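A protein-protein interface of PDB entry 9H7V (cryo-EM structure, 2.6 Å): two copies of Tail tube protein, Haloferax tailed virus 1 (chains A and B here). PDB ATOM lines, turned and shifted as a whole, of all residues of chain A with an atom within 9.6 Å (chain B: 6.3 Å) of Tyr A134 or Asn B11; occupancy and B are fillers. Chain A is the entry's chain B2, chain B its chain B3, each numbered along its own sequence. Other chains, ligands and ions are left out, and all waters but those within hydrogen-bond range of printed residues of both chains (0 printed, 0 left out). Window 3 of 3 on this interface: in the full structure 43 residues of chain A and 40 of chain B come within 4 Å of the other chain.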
ATOM      1  N   SER A 131      -2.993 -29.481  -2.852  1.00  0.00           N
ATOM      2  CA  SER A 131      -2.809 -29.812  -1.447  1.00  0.00           C
ATOM      3  C   SER A 131      -2.209 -28.616  -0.708  1.00  0.00           C
ATOM      4  O   SER A 131      -1.145 -28.717  -0.098  1.00  0.00           O
ATOM      5  CB  SER A 131      -1.974 -31.059  -1.301  1.00  0.00           C
ATOM      6  OG  SER A 131      -1.945 -31.493   0.050  1.00  0.00           O
ATOM      7  N   ALA A 132      -2.930 -27.490  -0.768  1.00  0.00           N
ATOM      8  CA  ALA A 132      -2.464 -26.209  -0.268  1.00  0.00           C
ATOM      9  C   ALA A 132      -2.769 -26.070   1.221  1.00  0.00           C
ATOM     10  O   ALA A 132      -3.875 -26.370   1.666  1.00  0.00           O
ATOM     11  CB  ALA A 132      -3.092 -25.093  -1.066  1.00  0.00           C
ATOM     12  N   THR A 133      -1.749 -25.639   1.974  1.00  0.00           N
ATOM     13  CA  THR A 133      -1.872 -25.159   3.342  1.00  0.00           C
ATOM     14  C   THR A 133      -1.097 -23.851   3.446  1.00  0.00           C
ATOM     15  O   THR A 133       0.033 -23.768   2.969  1.00  0.00           O
ATOM     16  CB  THR A 133      -1.339 -26.192   4.346  1.00  0.00           C
ATOM     17  OG1 THR A 133      -2.188 -27.340   4.305  1.00  0.00           O
ATOM     18  CG2 THR A 133      -1.257 -25.680   5.768  1.00  0.00           C
ATOM     19  N   TYR A 134      -1.705 -22.852   4.096  1.00  0.00           N
ATOM     20  CA  TYR A 134      -1.113 -21.535   4.262  1.00  0.00           C
ATOM     21  C   TYR A 134       0.304 -21.648   4.832  1.00  0.00           C
ATOM     22  O   TYR A 134       0.515 -22.294   5.857  1.00  0.00           O
ATOM     23  CB  TYR A 134      -2.013 -20.650   5.129  1.00  0.00           C
ATOM     24  CG  TYR A 134      -1.408 -19.310   5.455  1.00  0.00           C
ATOM     25  CD1 TYR A 134      -0.591 -19.149   6.565  1.00  0.00           C
ATOM     26  CD2 TYR A 134      -1.620 -18.211   4.635  1.00  0.00           C
ATOM     27  CE1 TYR A 134      -0.004 -17.928   6.859  1.00  0.00           C
ATOM     28  CE2 TYR A 134      -1.048 -16.981   4.920  1.00  0.00           C
ATOM     29  CZ  TYR A 134      -0.235 -16.840   6.033  1.00  0.00           C
ATOM     30  OH  TYR A 134       0.330 -15.633   6.322  1.00  0.00           O
ATOM     31  N   GLY A 135       1.259 -21.016   4.136  1.00  0.00           N
ATOM     32  CA  GLY A 135       2.637 -20.878   4.583  1.00  0.00           C
ATOM     33  C   GLY A 135       3.472 -22.144   4.397  1.00  0.00           C
ATOM     34  O   GLY A 135       4.489 -22.310   5.067  1.00  0.00           O
ATOM     35  N   GLU A 136       3.045 -23.018   3.474  1.00  0.00           N
ATOM     36  CA  GLU A 136       3.712 -24.289   3.230  1.00  0.00           C
ATOM     37  C   GLU A 136       3.783 -24.569   1.731  1.00  0.00           C
ATOM     38  O   GLU A 136       3.024 -23.997   0.952  1.00  0.00           O
ATOM     39  CB  GLU A 136       2.969 -25.428   3.933  1.00  0.00           C
ATOM     40  CG  GLU A 136       3.093 -25.400   5.445  1.00  0.00           C
ATOM     41  CD  GLU A 136       2.737 -26.691   6.164  1.00  0.00           C
ATOM     42  OE1 GLU A 136       1.748 -27.343   5.769  1.00  0.00           O
ATOM     43  OE2 GLU A 136       3.452 -27.039   7.124  1.00  0.00           O
ATOM     44  N   TYR A 137       4.719 -25.443   1.344  1.00  0.00           N
ATOM     45  CA  TYR A 137       4.744 -26.021   0.010  1.00  0.00           C
ATOM     46  C   TYR A 137       3.746 -27.172  -0.031  1.00  0.00           C
ATOM     47  O   TYR A 137       3.535 -27.838   0.982  1.00  0.00           O
ATOM     48  CB  TYR A 137       6.153 -26.493  -0.355  1.00  0.00           C
ATOM     49  CG  TYR A 137       7.165 -25.382  -0.464  1.00  0.00           C
ATOM     50  CD1 TYR A 137       7.864 -24.946   0.652  1.00  0.00           C
ATOM     51  CD2 TYR A 137       7.418 -24.758  -1.677  1.00  0.00           C
ATOM     52  CE1 TYR A 137       8.790 -23.917   0.567  1.00  0.00           C
ATOM     53  CE2 TYR A 137       8.343 -23.730  -1.779  1.00  0.00           C
ATOM     54  CZ  TYR A 137       9.030 -23.309  -0.653  1.00  0.00           C
ATOM     55  OH  TYR A 137       9.943 -22.298  -0.744  1.00  0.00           O
ATOM     56  N   GLU A 138       3.138 -27.386  -1.202  1.00  0.00           N
ATOM     57  CA  GLU A 138       2.108 -28.400  -1.360  1.00  0.00           C
ATOM     58  C   GLU A 138       2.725 -29.785  -1.178  1.00  0.00           C
ATOM     59  O   GLU A 138       3.711 -30.121  -1.834  1.00  0.00           O
ATOM     60  CB  GLU A 138       1.409 -28.264  -2.713  1.00  0.00           C
ATOM     61  CG  GLU A 138       0.592 -26.990  -2.848  1.00  0.00           C
ATOM     62  CD  GLU A 138      -0.514 -27.006  -3.892  1.00  0.00           C
ATOM     63  OE1 GLU A 138      -0.915 -28.106  -4.324  1.00  0.00           O
ATOM     64  OE2 GLU A 138      -0.982 -25.913  -4.262  1.00  0.00           O
ATOM     65  N   TRP B   9       3.947 -23.637  -4.231  1.00  0.00           N
ATOM     66  CA  TRP B   9       3.791 -22.842  -3.024  1.00  0.00           C
ATOM     67  C   TRP B   9       2.312 -22.509  -2.833  1.00  0.00           C
ATOM     68  O   TRP B   9       1.661 -22.038  -3.764  1.00  0.00           O
ATOM     69  CB  TRP B   9       4.672 -21.593  -3.146  1.00  0.00           C
ATOM     70  CG  TRP B   9       4.585 -20.593  -2.032  1.00  0.00           C
ATOM     71  CD1 TRP B   9       4.187 -19.294  -2.145  1.00  0.00           C
ATOM     72  CD2 TRP B   9       4.944 -20.783  -0.650  1.00  0.00           C
ATOM     73  NE1 TRP B   9       4.255 -18.663  -0.934  1.00  0.00           N
ATOM     74  CE2 TRP B   9       4.715 -19.550   0.004  1.00  0.00           C
ATOM     75  CE3 TRP B   9       5.424 -21.863   0.103  1.00  0.00           C
ATOM     76  CZ2 TRP B   9       4.948 -19.374   1.368  1.00  0.00           C
ATOM     77  CZ3 TRP B   9       5.656 -21.688   1.451  1.00  0.00           C
ATOM     78  CH2 TRP B   9       5.421 -20.459   2.073  1.00  0.00           C
ATOM     79  N   SER B  10       1.802 -22.762  -1.621  1.00  0.00           N
ATOM     80  CA  SER B  10       0.371 -22.755  -1.347  1.00  0.00           C
ATOM     81  C   SER B  10      -0.237 -21.361  -1.495  1.00  0.00           C
ATOM     82  O   SER B  10      -1.375 -21.238  -1.942  1.00  0.00           O
ATOM     83  CB  SER B  10       0.066 -23.337   0.002  1.00  0.00           C
ATOM     84  OG  SER B  10       0.543 -24.670   0.099  1.00  0.00           O
ATOM     85  N   ASN B  11       0.532 -20.325  -1.132  1.00  0.00           N
ATOM     86  CA  ASN B  11       0.043 -18.956  -1.085  1.00  0.00           C
ATOM     87  C   ASN B  11      -0.067 -18.355  -2.489  1.00  0.00           C
ATOM     88  O   ASN B  11      -0.600 -17.257  -2.643  1.00  0.00           O
ATOM     89  CB  ASN B  11       0.879 -18.094  -0.133  1.00  0.00           C
ATOM     90  CG  ASN B  11       0.693 -18.441   1.330  1.00  0.00           C
ATOM     91  OD1 ASN B  11       0.627 -19.611   1.702  1.00  0.00           O
ATOM     92  ND2 ASN B  11       0.632 -17.425   2.174  1.00  0.00           N
ATOM     93  N   SER B  12       0.418 -19.085  -3.504  1.00  0.00           N
ATOM     94  CA  SER B  12       0.422 -18.619  -4.882  1.00  0.00           C
ATOM     95  C   SER B  12      -0.868 -19.001  -5.611  1.00  0.00           C
ATOM     96  O   SER B  12      -1.104 -18.532  -6.723  1.00  0.00           O
ATOM     97  CB  SER B  12       1.641 -19.121  -5.615  1.00  0.00           C
ATOM     98  OG  SER B  12       2.825 -18.576  -5.056  1.00  0.00           O
ATOM     99  N   GLY B  13      -1.700 -19.837  -4.976  1.00  0.00           N
ATOM    100  CA  GLY B  13      -2.907 -20.361  -5.600  1.00  0.00           C
ATOM    101  C   GLY B  13      -4.044 -19.344  -5.630  1.00  0.00           C
ATOM    102  O   GLY B  13      -4.325 -18.697  -4.622  1.00  0.00           O
ATOM    103  N   ALA B  14      -4.688 -19.220  -6.799  1.00  0.00           N
ATOM    104  CA  ALA B  14      -5.889 -18.417  -6.966  1.00  0.00           C
ATOM    105  C   ALA B  14      -7.089 -19.341  -7.166  1.00  0.00           C
ATOM    106  O   ALA B  14      -7.133 -20.097  -8.135  1.00  0.00           O
ATOM    107  CB  ALA B  14      -5.716 -17.460  -8.121  1.00  0.00           C
ATOM    108  N   VAL B  31      -8.726 -17.735   1.331  1.00  0.00           N
ATOM    109  CA  VAL B  31      -8.432 -19.158   1.414  1.00  0.00           C
ATOM    110  C   VAL B  31      -7.199 -19.366   2.292  1.00  0.00           C
ATOM    111  O   VAL B  31      -6.263 -18.569   2.250  1.00  0.00           O
ATOM    112  CB  VAL B  31      -8.242 -19.742  -0.001  1.00  0.00           C
ATOM    113  CG1 VAL B  31      -7.481 -21.058  -0.011  1.00  0.00           C
ATOM    114  CG2 VAL B  31      -9.562 -19.879  -0.742  1.00  0.00           C
ATOM    115  N   ARG B  32      -7.218 -20.454   3.077  1.00  0.00           N
ATOM    116  CA  ARG B  32      -6.101 -20.846   3.923  1.00  0.00           C
ATOM    117  C   ARG B  32      -5.639 -22.265   3.580  1.00  0.00           C
ATOM    118  O   ARG B  32      -4.445 -22.550   3.655  1.00  0.00           O
ATOM    119  CB  ARG B  32      -6.444 -20.672   5.408  1.00  0.00           C
ATOM    120  CG  ARG B  32      -6.872 -19.259   5.781  1.00  0.00           C
ATOM    121  CD  ARG B  32      -6.667 -18.874   7.232  1.00  0.00           C
ATOM    122  NE  ARG B  32      -5.260 -18.644   7.533  1.00  0.00           N
ATOM    123  CZ  ARG B  32      -4.592 -19.172   8.554  1.00  0.00           C
ATOM    124  NH1 ARG B  32      -3.312 -18.888   8.716  1.00  0.00           N
ATOM    125  NH2 ARG B  32      -5.200 -19.963   9.423  1.00  0.00           N
ATOM    126  N   ASP B  33      -6.586 -23.144   3.217  1.00  0.00           N
ATOM    127  CA  ASP B  33      -6.281 -24.503   2.787  1.00  0.00           C
ATOM    128  C   ASP B  33      -7.192 -24.902   1.628  1.00  0.00           C
ATOM    129  O   ASP B  33      -8.361 -24.520   1.609  1.00  0.00           O
ATOM    130  CB  ASP B  33      -6.464 -25.520   3.919  1.00  0.00           C
ATOM    131  CG  ASP B  33      -5.533 -25.339   5.106  1.00  0.00           C
ATOM    132  OD1 ASP B  33      -5.768 -24.407   5.901  1.00  0.00           O
ATOM    133  OD2 ASP B  33      -4.591 -26.144   5.238  1.00  0.00           O
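N of Ser A131 lies within hydrogen-bond range of OE1 of Glu A138, 2.9 Å away.
No position is printed for both chains.
Of the 13 pairs that touch across the chains among the printed residues, none has its exchanged pair printed and touching as well.
Tyr A134 touches two residues of chain B.
No residue of chain A comes within 4 Å of Ser B12.
No residue of chain A comes within 4 Å of Gly B13.
Printed residues of chain B within 4 Å of Glu A136: Trp B9 and Ser B10.
Of the printed residues of chain B, Thr A133 touches Ser B10 (3.0 Å), Arg B32 (3.6 Å) and Asp B33 (2.8 Å).
Of the printed residues of chain B, Ala A132 touches Ser B10 (3.4 Å) and Asp B33 (3.2 Å).
Printed residues of chain A within 4 Å of Arg B32: Thr A133 and Tyr A134.
Val B31 touches none of the printed residues of chain A.
Of the 9 printed residues of chain B, 5 touch a printed residue of chain A.
Printed residues of chain B that touch a printed residue of chain A: Trp B9, Ser B10, Asn B11, Arg B32 and Asp B33.
Hydrophobic or aromatic side chains of chain B within 4 Å of the printed part of chain A: Trp B9.
Of the 8 printed residues of chain A, 7 touch a printed residue of chain B.
Printed residues of chain A that touch a printed residue of chain B: Ala A132, Thr A133, Tyr A134, Gly A135, Glu A136, Tyr A137 and Glu A138.
Ala A132 touches Ser B10 (CA to OG, 3.4 Å).
Asp B33 touches Ala A132.
O of Arg B32 touches C of Thr A133 (3.6 Å).
ND2 of Asn B11 touches CE2 of Tyr A134 (3.2 Å).
CH2 of Trp B9 touches C of Gly A135 (3.5 Å).
Glu A136 touches Trp B9.
Tyr A137 touches Trp B9 (N to CE3, 3.9 Å).
OG of Ser B10 touches CG of Glu A138, at 3.8 Å.
O of Thr A133 sits close to OG of Ser B10 (3.1 Å).
The side-chain carboxylate of Asp B33 sits at hydrogen-bond distance from the side-chain hydroxyl of Thr A133, at 2.8 Å.
N of Tyr A134 lies within hydrogen-bond range of O of Arg B32.
The backbone NH of Gly A135 lies within hydrogen-bond range of the side-chain amide oxygen of Asn B11 (2.9 Å).
The backbone carbonyl oxygen (O) of Glu A136 lies within hydrogen-bond range of the side-chain hydroxyl (OG) of Ser B10 (2.7 Å).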
